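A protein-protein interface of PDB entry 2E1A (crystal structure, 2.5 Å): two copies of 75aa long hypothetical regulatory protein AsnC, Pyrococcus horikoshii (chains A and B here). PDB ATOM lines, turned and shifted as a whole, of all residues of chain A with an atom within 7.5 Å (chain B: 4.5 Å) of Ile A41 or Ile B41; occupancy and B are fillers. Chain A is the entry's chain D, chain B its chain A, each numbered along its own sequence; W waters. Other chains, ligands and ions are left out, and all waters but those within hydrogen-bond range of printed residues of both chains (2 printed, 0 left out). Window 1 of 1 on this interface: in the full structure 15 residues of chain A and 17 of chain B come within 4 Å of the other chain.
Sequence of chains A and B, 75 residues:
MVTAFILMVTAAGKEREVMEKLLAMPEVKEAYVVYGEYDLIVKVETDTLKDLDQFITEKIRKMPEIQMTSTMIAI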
ATOM      1  N   ALA A   4     -27.136   7.418  13.451  1.00  0.00           N
ATOM      2  CA  ALA A   4     -26.925   6.731  14.723  1.00  0.00           C
ATOM      3  C   ALA A   4     -25.532   6.995  15.301  1.00  0.00           C
ATOM      4  O   ALA A   4     -24.591   7.303  14.572  1.00  0.00           O
ATOM      5  CB  ALA A   4     -27.146   5.235  14.549  1.00  0.00           C
ATOM      6  N   PHE A   5     -25.416   6.895  16.621  1.00  0.00           N
ATOM      7  CA  PHE A   5     -24.139   7.090  17.290  1.00  0.00           C
ATOM      8  C   PHE A   5     -23.772   5.788  17.966  1.00  0.00           C
ATOM      9  O   PHE A   5     -24.549   5.250  18.755  1.00  0.00           O
ATOM     10  CB  PHE A   5     -24.214   8.192  18.348  1.00  0.00           C
ATOM     11  CG  PHE A   5     -24.355   9.567  17.782  1.00  0.00           C
ATOM     12  CD1 PHE A   5     -25.598  10.034  17.368  1.00  0.00           C
ATOM     13  CD2 PHE A   5     -23.237  10.383  17.622  1.00  0.00           C
ATOM     14  CE1 PHE A   5     -25.732  11.295  16.803  1.00  0.00           C
ATOM     15  CE2 PHE A   5     -23.355  11.648  17.059  1.00  0.00           C
ATOM     16  CZ  PHE A   5     -24.605  12.109  16.644  1.00  0.00           C
ATOM     17  N   ILE A   6     -22.584   5.285  17.656  1.00  0.00           N
ATOM     18  CA  ILE A   6     -22.119   4.038  18.240  1.00  0.00           C
ATOM     19  C   ILE A   6     -21.047   4.289  19.288  1.00  0.00           C
ATOM     20  O   ILE A   6     -20.038   4.944  19.015  1.00  0.00           O
ATOM     21  CB  ILE A   6     -21.508   3.109  17.174  1.00  0.00           C
ATOM     22  CG1 ILE A   6     -22.438   3.005  15.972  1.00  0.00           C
ATOM     23  CG2 ILE A   6     -21.292   1.718  17.763  1.00  0.00           C
ATOM     24  CD1 ILE A   6     -21.785   2.362  14.777  1.00  0.00           C
ATOM     25  N   LEU A   7     -21.278   3.776  20.490  1.00  0.00           N
ATOM     26  CA  LEU A   7     -20.314   3.896  21.571  1.00  0.00           C
ATOM     27  C   LEU A   7     -19.567   2.572  21.501  1.00  0.00           C
ATOM     28  O   LEU A   7     -20.186   1.510  21.558  1.00  0.00           O
ATOM     29  CB  LEU A   7     -21.040   4.053  22.909  1.00  0.00           C
ATOM     30  CG  LEU A   7     -21.908   5.321  22.987  1.00  0.00           C
ATOM     31  CD1 LEU A   7     -22.809   5.303  24.223  1.00  0.00           C
ATOM     32  CD2 LEU A   7     -20.996   6.533  22.984  1.00  0.00           C
ATOM     33  N   MET A   8     -18.247   2.620  21.353  1.00  0.00           N
ATOM     34  CA  MET A   8     -17.487   1.383  21.229  1.00  0.00           C
ATOM     35  C   MET A   8     -16.357   1.191  22.236  1.00  0.00           C
ATOM     36  O   MET A   8     -15.670   2.136  22.627  1.00  0.00           O
ATOM     37  CB  MET A   8     -16.906   1.273  19.814  1.00  0.00           C
ATOM     38  CG  MET A   8     -17.907   1.569  18.694  1.00  0.00           C
ATOM     39  SD  MET A   8     -17.221   1.388  17.002  1.00  0.00           S
ATOM     40  CE  MET A   8     -15.538   1.778  17.320  1.00  0.00           C
ATOM     41  N   MET A  19     -10.220   3.427  14.618  1.00  0.00           N
ATOM     42  CA  MET A  19     -10.815   4.668  14.135  1.00  0.00           C
ATOM     43  C   MET A  19     -10.456   4.914  12.677  1.00  0.00           C
ATOM     44  O   MET A  19     -11.300   5.327  11.886  1.00  0.00           O
ATOM     45  CB  MET A  19     -10.345   5.850  14.973  1.00  0.00           C
ATOM     46  CG  MET A  19     -10.734   7.191  14.387  1.00  0.00           C
ATOM     47  SD  MET A  19     -10.296   8.534  15.479  1.00  0.00           S
ATOM     48  CE  MET A  19     -11.595   8.375  16.580  1.00  0.00           C
ATOM     49  N   LEU A  22     -12.608   2.844  10.568  1.00  0.00           N
ATOM     50  CA  LEU A  22     -13.953   3.397  10.553  1.00  0.00           C
ATOM     51  C   LEU A  22     -14.056   4.615   9.650  1.00  0.00           C
ATOM     52  O   LEU A  22     -14.967   4.713   8.823  1.00  0.00           O
ATOM     53  CB  LEU A  22     -14.383   3.770  11.973  1.00  0.00           C
ATOM     54  CG  LEU A  22     -14.431   2.577  12.932  1.00  0.00           C
ATOM     55  CD1 LEU A  22     -14.764   3.042  14.330  1.00  0.00           C
ATOM     56  CD2 LEU A  22     -15.452   1.577  12.436  1.00  0.00           C
ATOM     57  N   VAL A  28     -19.595   5.985   8.002  1.00  0.00           N
ATOM     58  CA  VAL A  28     -19.081   6.781   9.105  1.00  0.00           C
ATOM     59  C   VAL A  28     -18.935   8.264   8.758  1.00  0.00           C
ATOM     60  O   VAL A  28     -18.235   8.623   7.816  1.00  0.00           O
ATOM     61  CB  VAL A  28     -17.725   6.213   9.562  1.00  0.00           C
ATOM     62  CG1 VAL A  28     -17.205   6.975  10.765  1.00  0.00           C
ATOM     63  CG2 VAL A  28     -17.882   4.731   9.886  1.00  0.00           C
ATOM     64  N   GLU A  30     -18.452  10.657  11.478  1.00  0.00           N
ATOM     65  CA  GLU A  30     -17.557  11.203  12.497  1.00  0.00           C
ATOM     66  C   GLU A  30     -17.074  10.071  13.396  1.00  0.00           C
ATOM     67  O   GLU A  30     -17.795   9.104  13.635  1.00  0.00           O
ATOM     68  CB  GLU A  30     -18.277  12.256  13.352  1.00  0.00           C
ATOM     69  CG  GLU A  30     -19.000  13.325  12.554  1.00  0.00           C
ATOM     70  CD  GLU A  30     -19.666  14.396  13.413  1.00  0.00           C
ATOM     71  OE1 GLU A  30     -20.557  15.088  12.883  1.00  0.00           O
ATOM     72  OE2 GLU A  30     -19.301  14.566  14.597  1.00  0.00           O
ATOM     73  N   ALA A  31     -15.839  10.173  13.869  1.00  0.00           N
ATOM     74  CA  ALA A  31     -15.301   9.170  14.775  1.00  0.00           C
ATOM     75  C   ALA A  31     -14.346   9.894  15.703  1.00  0.00           C
ATOM     76  O   ALA A  31     -13.550  10.724  15.263  1.00  0.00           O
ATOM     77  CB  ALA A  31     -14.588   8.077  14.014  1.00  0.00           C
ATOM     78  N   TYR A  32     -14.443   9.591  16.991  1.00  0.00           N
ATOM     79  CA  TYR A  32     -13.597  10.234  17.990  1.00  0.00           C
ATOM     80  C   TYR A  32     -13.128   9.243  19.039  1.00  0.00           C
ATOM     81  O   TYR A  32     -13.896   8.387  19.482  1.00  0.00           O
ATOM     82  CB  TYR A  32     -14.378  11.328  18.712  1.00  0.00           C
ATOM     83  CG  TYR A  32     -14.668  12.564  17.907  1.00  0.00           C
ATOM     84  CD1 TYR A  32     -13.783  13.637  17.918  1.00  0.00           C
ATOM     85  CD2 TYR A  32     -15.861  12.694  17.192  1.00  0.00           C
ATOM     86  CE1 TYR A  32     -14.075  14.813  17.251  1.00  0.00           C
ATOM     87  CE2 TYR A  32     -16.166  13.868  16.514  1.00  0.00           C
ATOM     88  CZ  TYR A  32     -15.266  14.929  16.555  1.00  0.00           C
ATOM     89  OH  TYR A  32     -15.565  16.125  15.941  1.00  0.00           O
ATOM     90  N   VAL A  33     -11.865   9.359  19.431  1.00  0.00           N
ATOM     91  CA  VAL A  33     -11.343   8.516  20.494  1.00  0.00           C
ATOM     92  C   VAL A  33     -11.697   9.348  21.725  1.00  0.00           C
ATOM     93  O   VAL A  33     -11.428  10.546  21.752  1.00  0.00           O
ATOM     94  CB  VAL A  33      -9.808   8.350  20.399  1.00  0.00           C
ATOM     95  CG1 VAL A  33      -9.309   7.479  21.553  1.00  0.00           C
ATOM     96  CG2 VAL A  33      -9.431   7.733  19.047  1.00  0.00           C
ATOM     97  N   VAL A  34     -12.331   8.744  22.722  1.00  0.00           N
ATOM     98  CA  VAL A  34     -12.705   9.509  23.907  1.00  0.00           C
ATOM     99  C   VAL A  34     -12.205   8.911  25.206  1.00  0.00           C
ATOM    100  O   VAL A  34     -11.806   7.744  25.274  1.00  0.00           O
ATOM    101  CB  VAL A  34     -14.245   9.677  24.033  1.00  0.00           C
ATOM    102  CG1 VAL A  34     -14.776  10.519  22.881  1.00  0.00           C
ATOM    103  CG2 VAL A  34     -14.920   8.303  24.067  1.00  0.00           C
ATOM    104  N   TYR A  38     -16.297   4.368  27.419  1.00  0.00           N
ATOM    105  CA  TYR A  38     -16.162   3.964  26.028  1.00  0.00           C
ATOM    106  C   TYR A  38     -14.888   4.523  25.406  1.00  0.00           C
ATOM    107  O   TYR A  38     -14.431   5.601  25.778  1.00  0.00           O
ATOM    108  CB  TYR A  38     -17.403   4.425  25.261  1.00  0.00           C
ATOM    109  CG  TYR A  38     -18.660   3.689  25.693  1.00  0.00           C
ATOM    110  CD1 TYR A  38     -18.885   2.373  25.293  1.00  0.00           C
ATOM    111  CD2 TYR A  38     -19.611   4.300  26.512  1.00  0.00           C
ATOM    112  CE1 TYR A  38     -20.019   1.679  25.694  1.00  0.00           C
ATOM    113  CE2 TYR A  38     -20.756   3.612  26.923  1.00  0.00           C
ATOM    114  CZ  TYR A  38     -20.951   2.302  26.508  1.00  0.00           C
ATOM    115  OH  TYR A  38     -22.071   1.601  26.895  1.00  0.00           O
ATOM    116  N   ASP A  39     -14.309   3.786  24.467  1.00  0.00           N
ATOM    117  CA  ASP A  39     -13.077   4.221  23.818  1.00  0.00           C
ATOM    118  C   ASP A  39     -13.326   5.059  22.583  1.00  0.00           C
ATOM    119  O   ASP A  39     -12.516   5.916  22.228  1.00  0.00           O
ATOM    120  CB  ASP A  39     -12.238   3.014  23.422  1.00  0.00           C
ATOM    121  CG  ASP A  39     -11.948   2.122  24.590  1.00  0.00           C
ATOM    122  OD1 ASP A  39     -11.422   2.634  25.601  1.00  0.00           O
ATOM    123  OD2 ASP A  39     -12.251   0.914  24.504  1.00  0.00           O
ATOM    124  N   LEU A  40     -14.452   4.806  21.927  1.00  0.00           N
ATOM    125  CA  LEU A  40     -14.792   5.522  20.712  1.00  0.00           C
ATOM    126  C   LEU A  40     -16.259   5.894  20.612  1.00  0.00           C
ATOM    127  O   LEU A  40     -17.131   5.182  21.105  1.00  0.00           O
ATOM    128  CB  LEU A  40     -14.445   4.665  19.491  1.00  0.00           C
ATOM    129  CG  LEU A  40     -12.993   4.402  19.079  1.00  0.00           C
ATOM    130  CD1 LEU A  40     -12.959   3.330  18.015  1.00  0.00           C
ATOM    131  CD2 LEU A  40     -12.363   5.678  18.541  1.00  0.00           C
ATOM    132  N   ILE A  41     -16.520   7.035  19.988  1.00  0.00           N
ATOM    133  CA  ILE A  41     -17.880   7.453  19.722  1.00  0.00           C
ATOM    134  C   ILE A  41     -17.867   7.676  18.212  1.00  0.00           C
ATOM    135  O   ILE A  41     -17.021   8.394  17.679  1.00  0.00           O
ATOM    136  CB  ILE A  41     -18.303   8.733  20.474  1.00  0.00           C
ATOM    137  CG1 ILE A  41     -19.791   8.980  20.197  1.00  0.00           C
ATOM    138  CG2 ILE A  41     -17.479   9.928  20.028  1.00  0.00           C
ATOM    139  CD1 ILE A  41     -20.411  10.091  21.009  1.00  0.00           C
ATOM    140  N   VAL A  42     -18.789   7.020  17.519  1.00  0.00           N
ATOM    141  CA  VAL A  42     -18.843   7.100  16.071  1.00  0.00           C
ATOM    142  C   VAL A  42     -20.221   7.487  15.556  1.00  0.00           C
ATOM    143  O   VAL A  42     -21.232   6.920  15.982  1.00  0.00           O
ATOM    144  CB  VAL A  42     -18.450   5.738  15.469  1.00  0.00           C
ATOM    145  CG1 VAL A  42     -18.153   5.880  13.985  1.00  0.00           C
ATOM    146  CG2 VAL A  42     -17.243   5.161  16.228  1.00  0.00           C
ATOM    147  N   LYS A  43     -20.265   8.462  14.650  1.00  0.00           N
ATOM    148  CA  LYS A  43     -21.531   8.893  14.063  1.00  0.00           C
ATOM    149  C   LYS A  43     -21.651   8.224  12.713  1.00  0.00           C
ATOM    150  O   LYS A  43     -20.745   8.326  11.887  1.00  0.00           O
ATOM    151  CB  LYS A  43     -21.565  10.403  13.855  1.00  0.00           C
ATOM    152  CG  LYS A  43     -22.881  10.917  13.236  1.00  0.00           C
ATOM    153  CD  LYS A  43     -22.781  12.404  12.974  1.00  0.00           C
ATOM    154  CE  LYS A  43     -24.103  13.009  12.589  1.00  0.00           C
ATOM    155  NZ  LYS A  43     -23.911  14.446  12.268  1.00  0.00           N
ATOM    156  N   MET A  72     -26.947   4.080  19.348  1.00  0.00           N
ATOM    157  CA  MET A  72     -28.068   4.925  19.706  1.00  0.00           C
ATOM    158  C   MET A  72     -28.613   5.560  18.452  1.00  0.00           C
ATOM    159  O   MET A  72     -28.008   6.480  17.897  1.00  0.00           O
ATOM    160  CB  MET A  72     -27.608   6.006  20.673  1.00  0.00           C
ATOM    161  CG  MET A  72     -26.927   5.447  21.901  1.00  0.00           C
ATOM    162  SD  MET A  72     -26.122   6.723  22.888  1.00  0.00           S
ATOM    163  CE  MET A  72     -27.016   6.525  24.402  1.00  0.00           C
ATOM    164  N   ALA A  74     -30.894   7.847  16.165  1.00  0.00           N
ATOM    165  CA  ALA A  74     -31.448   9.191  16.324  1.00  0.00           C
ATOM    166  C   ALA A  74     -32.850   9.327  15.742  1.00  0.00           C
ATOM    167  O   ALA A  74     -33.211   8.623  14.798  1.00  0.00           O
ATOM    168  CB  ALA A  74     -30.524  10.207  15.664  1.00  0.00           C
ATOM    169  N   PHE B   5     -18.683  15.076  23.946  1.00  0.00           N
ATOM    170  CA  PHE B   5     -20.044  14.643  23.698  1.00  0.00           C
ATOM    171  C   PHE B   5     -20.703  14.436  25.047  1.00  0.00           C
ATOM    172  O   PHE B   5     -20.146  13.779  25.930  1.00  0.00           O
ATOM    173  CB  PHE B   5     -20.079  13.329  22.919  1.00  0.00           C
ATOM    174  CG  PHE B   5     -19.712  13.471  21.469  1.00  0.00           C
ATOM    175  CD1 PHE B   5     -18.374  13.514  21.074  1.00  0.00           C
ATOM    176  CD2 PHE B   5     -20.706  13.582  20.494  1.00  0.00           C
ATOM    177  CE1 PHE B   5     -18.030  13.665  19.730  1.00  0.00           C
ATOM    178  CE2 PHE B   5     -20.379  13.733  19.146  1.00  0.00           C
ATOM    179  CZ  PHE B   5     -19.033  13.774  18.762  1.00  0.00           C
ATOM    180  N   ILE B   6     -21.885  15.010  25.207  1.00  0.00           N
ATOM    181  CA  ILE B   6     -22.615  14.877  26.446  1.00  0.00           C
ATOM    182  C   ILE B   6     -23.890  14.080  26.169  1.00  0.00           C
ATOM    183  O   ILE B   6     -24.709  14.472  25.330  1.00  0.00           O
ATOM    184  CB  ILE B   6     -22.968  16.268  27.026  1.00  0.00           C
ATOM    185  CG1 ILE B   6     -21.709  17.146  27.080  1.00  0.00           C
ATOM    186  CG2 ILE B   6     -23.523  16.114  28.433  1.00  0.00           C
ATOM    187  CD1 ILE B   6     -21.965  18.588  27.545  1.00  0.00           C
ATOM    188  N   LEU B   7     -24.032  12.940  26.838  1.00  0.00           N
ATOM    189  CA  LEU B   7     -25.217  12.106  26.673  1.00  0.00           C
ATOM    190  C   LEU B   7     -26.096  12.497  27.837  1.00  0.00           C
ATOM    191  O   LEU B   7     -25.612  12.635  28.957  1.00  0.00           O
ATOM    192  CB  LEU B   7     -24.871  10.621  26.777  1.00  0.00           C
ATOM    193  CG  LEU B   7     -23.678  10.089  25.978  1.00  0.00           C
ATOM    194  CD1 LEU B   7     -23.878   8.605  25.732  1.00  0.00           C
ATOM    195  CD2 LEU B   7     -23.542  10.824  24.667  1.00  0.00           C
ATOM    196  N   GLU B  30     -23.842  20.044  17.555  1.00  0.00           N
ATOM    197  CA  GLU B  30     -24.850  19.083  17.109  1.00  0.00           C
ATOM    198  C   GLU B  30     -25.654  18.599  18.309  1.00  0.00           C
ATOM    199  O   GLU B  30     -25.168  18.603  19.439  1.00  0.00           O
ATOM    200  CB  GLU B  30     -24.211  17.861  16.447  1.00  0.00           C
ATOM    201  CG  GLU B  30     -23.115  18.169  15.465  1.00  0.00           C
ATOM    202  CD  GLU B  30     -22.464  16.909  14.930  1.00  0.00           C
ATOM    203  OE1 GLU B  30     -21.376  17.020  14.316  1.00  0.00           O
ATOM    204  OE2 GLU B  30     -23.048  15.820  15.121  1.00  0.00           O
ATOM    205  N   ALA B  31     -26.884  18.173  18.050  1.00  0.00           N
ATOM    206  CA  ALA B  31     -27.743  17.668  19.102  1.00  0.00           C
ATOM    207  C   ALA B  31     -28.777  16.754  18.466  1.00  0.00           C
ATOM    208  O   ALA B  31     -29.377  17.083  17.444  1.00  0.00           O
ATOM    209  CB  ALA B  31     -28.409  18.814  19.839  1.00  0.00           C
ATOM    210  N   TYR B  32     -28.961  15.591  19.072  1.00  0.00           N
ATOM    211  CA  TYR B  32     -29.902  14.607  18.564  1.00  0.00           C
ATOM    212  C   TYR B  32     -30.657  13.933  19.684  1.00  0.00           C
ATOM    213  O   TYR B  32     -30.086  13.648  20.745  1.00  0.00           O
ATOM    214  CB  TYR B  32     -29.162  13.504  17.808  1.00  0.00           C
ATOM    215  CG  TYR B  32     -28.596  13.894  16.462  1.00  0.00           C
ATOM    216  CD1 TYR B  32     -29.351  13.731  15.298  1.00  0.00           C
ATOM    217  CD2 TYR B  32     -27.289  14.379  16.342  1.00  0.00           C
ATOM    218  CE1 TYR B  32     -28.821  14.031  14.051  1.00  0.00           C
ATOM    219  CE2 TYR B  32     -26.747  14.685  15.099  1.00  0.00           C
ATOM    220  CZ  TYR B  32     -27.521  14.506  13.957  1.00  0.00           C
ATOM    221  OH  TYR B  32     -27.002  14.798  12.719  1.00  0.00           O
ATOM    222  N   VAL B  34     -32.103  10.641  20.931  1.00  0.00           N
ATOM    223  CA  VAL B  34     -31.757   9.259  20.588  1.00  0.00           C
ATOM    224  C   VAL B  34     -32.530   8.192  21.372  1.00  0.00           C
ATOM    225  O   VAL B  34     -33.135   8.483  22.391  1.00  0.00           O
ATOM    226  CB  VAL B  34     -30.248   9.004  20.805  1.00  0.00           C
ATOM    227  CG1 VAL B  34     -29.417   9.767  19.755  1.00  0.00           C
ATOM    228  CG2 VAL B  34     -29.856   9.435  22.224  1.00  0.00           C
ATOM    229  N   LEU B  40     -30.724  12.322  24.799  1.00  0.00           N
ATOM    230  CA  LEU B  40     -30.090  13.314  23.944  1.00  0.00           C
ATOM    231  C   LEU B  40     -28.586  13.118  23.899  1.00  0.00           C
ATOM    232  O   LEU B  40     -27.980  12.674  24.872  1.00  0.00           O
ATOM    233  CB  LEU B  40     -30.358  14.737  24.461  1.00  0.00           C
ATOM    234  CG  LEU B  40     -31.741  15.391  24.501  1.00  0.00           C
ATOM    235  CD1 LEU B  40     -31.636  16.707  25.240  1.00  0.00           C
ATOM    236  CD2 LEU B  40     -32.261  15.629  23.099  1.00  0.00           C
ATOM    237  N   ILE B  41     -27.991  13.419  22.750  1.00  0.00           N
ATOM    238  CA  ILE B  41     -26.546  13.371  22.620  1.00  0.00           C
ATOM    239  C   ILE B  41     -26.224  14.739  22.056  1.00  0.00           C
ATOM    240  O   ILE B  41     -26.853  15.190  21.095  1.00  0.00           O
ATOM    241  CB  ILE B  41     -26.026  12.260  21.676  1.00  0.00           C
ATOM    242  CG1 ILE B  41     -24.508  12.403  21.533  1.00  0.00           C
ATOM    243  CG2 ILE B  41     -26.666  12.357  20.318  1.00  0.00           C
ATOM    244  CD1 ILE B  41     -23.806  11.121  21.150  1.00  0.00           C
ATOM    245  N   VAL B  42     -25.276  15.412  22.691  1.00  0.00           N
ATOM    246  CA  VAL B  42     -24.883  16.744  22.284  1.00  0.00           C
ATOM    247  C   VAL B  42     -23.380  16.810  22.089  1.00  0.00           C
ATOM    248  O   VAL B  42     -22.612  16.262  22.878  1.00  0.00           O
ATOM    249  CB  VAL B  42     -25.289  17.773  23.358  1.00  0.00           C
ATOM    250  CG1 VAL B  42     -24.945  19.168  22.905  1.00  0.00           C
ATOM    251  CG2 VAL B  42     -26.782  17.665  23.640  1.00  0.00           C
ATOM    252  N   LYS B  43     -22.957  17.471  21.024  1.00  0.00           N
ATOM    253  CA  LYS B  43     -21.541  17.618  20.768  1.00  0.00           C
ATOM    254  C   LYS B  43     -21.214  19.077  21.020  1.00  0.00           C
ATOM    255  O   LYS B  43     -21.850  19.971  20.452  1.00  0.00           O
ATOM    256  CB  LYS B  43     -21.213  17.243  19.330  1.00  0.00           C
ATOM    257  CG  LYS B  43     -19.747  17.392  18.960  1.00  0.00           C
ATOM    258  CD  LYS B  43     -19.604  17.186  17.467  1.00  0.00           C
ATOM    259  CE  LYS B  43     -18.277  17.645  16.951  1.00  0.00           C
ATOM    260  NZ  LYS B  43     -18.274  17.554  15.476  1.00  0.00           N
HETATM  261  O   HOH W   1     -25.297  16.809  10.459  1.00  0.00           O
HETATM  262  O   HOH W   2     -23.667  17.878  11.986  1.00  0.00           O
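Ile B41 touches two residues of chain A.
Of the printed residues of chain A, Leu B7 touches Leu A7 (3.8 Å) and Met A72 (3.99 Å).
Printed residues of chain B within 4 Å of Leu A7: Leu B7.
Printed residues of chain B within 4 Å of Lys A43: Glu B30 and Tyr B32.
Of the printed residues of chain B, Met A72 touches Leu B7 and Val B34.
Of the printed residues of chain B, Tyr A32 touches Phe B5 (3.5 Å) and Lys B43 (3.1 Å).
Ala B31 touches none of the printed residues of chain A.
The nearest residue of chain A that does not touch Ile B41 is Met A72 (5.3 Å).
Water W1 bridges the side-chain amino group (NZ) of Lys A43 (3.3 Å) and the side-chain hydroxyl (OH) of Tyr B32 (3.5 Å).
Water W2 lies within hydrogen-bond range of the side-chain carboxylate (OE1) of Glu B30 (3.4 Å) and the side-chain amino group (NZ) of Lys A43 (3.5 Å).
Printed residues of chain B that touch a printed residue of chain A: Phe B5, Leu B7, Glu B30, Tyr B32, Val B34, Ile B41 and Lys B43.
Hydrophobic or aromatic side chains of chain A within 4 Å of the printed part of chain B: Phe A5, Leu A7, Tyr A32, Ile A41, Met A72 and Ala A74.
Along chain A the printed residues that touch a printed residue of chain B span positions 5 to 74.
The side-chain carboxylate (OE1) of Glu B30 lies close to the side-chain carboxylate (OE1) of Glu A30.
The side-chain carboxylate (OE2) of Glu B30 lies within salt-bridge range of the side-chain amino group (NZ) of Lys A43, at 3.3 Å.
The side-chain hydroxyl of Tyr B32 sits at hydrogen-bond distance from the side-chain amino group of Lys A43 (3.1 Å).
NZ of Lys B43 is in salt-bridge range of OE2 of Glu A30, 3.3 Å away.
The side-chain amino group of Lys B43 sits at hydrogen-bond distance from the side-chain hydroxyl of Tyr A32 (3.1 Å).
NZ of Lys B43 is in salt-bridge range of OE1 of Glu B30 (3.4 Å).
The backbone carbonyl oxygen (O) of Tyr B32 sits at hydrogen-bond distance from the backbone NH (N) of Ile B41, at 2.9 Å.
The backbone carbonyl oxygen (O) of Phe A5 is in hydrogen-bond range of the backbone NH (N) of Met A72.
The side-chain carboxylate (OE1) of Glu A30 is in salt-bridge range of the side-chain amino group (NZ) of Lys A43, 3.5 Å away.
The backbone NH of Tyr A32 sits at hydrogen-bond distance from the backbone carbonyl oxygen of Ile A41 (2.9 Å).
Among the printed residues, pairs that only touch across the chains: Tyr A32 with Phe B5 (3.5 Å), Ile A41 with Phe B5 (3.5 Å), Phe A5 with Tyr B32 (3.5 Å), Ile A41 with Ile B41 (3.6 Å), Phe A5 with Ile B41 (3.6 Å), Ala A74 with Tyr B32 (3.7 Å), Leu A7 with Leu B7 (3.8 Å), Met A72 with Leu B7 (3.99 Å) and Met A72 with Val B34 (3.997 Å).
Phe A5 touches Tyr B32, and with the chains exchanged Tyr A32 touches Phe B5.
Phe A5 touches Ile B41, and with the chains exchanged Ile A41 touches Phe B5.
Leu A7 touches its own counterpart, Leu B7.
Glu A30 touches Lys B43, and with the chains exchanged Lys A43 touches Glu B30.
Positions printed for both chains: 5, 6, 7, 30, 31, 32, 34, 40, 41, 42 and 43.
Of the 14 pairs that touch across the chains among the printed residues, 11 have their exchanged pair printed and touching as well.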
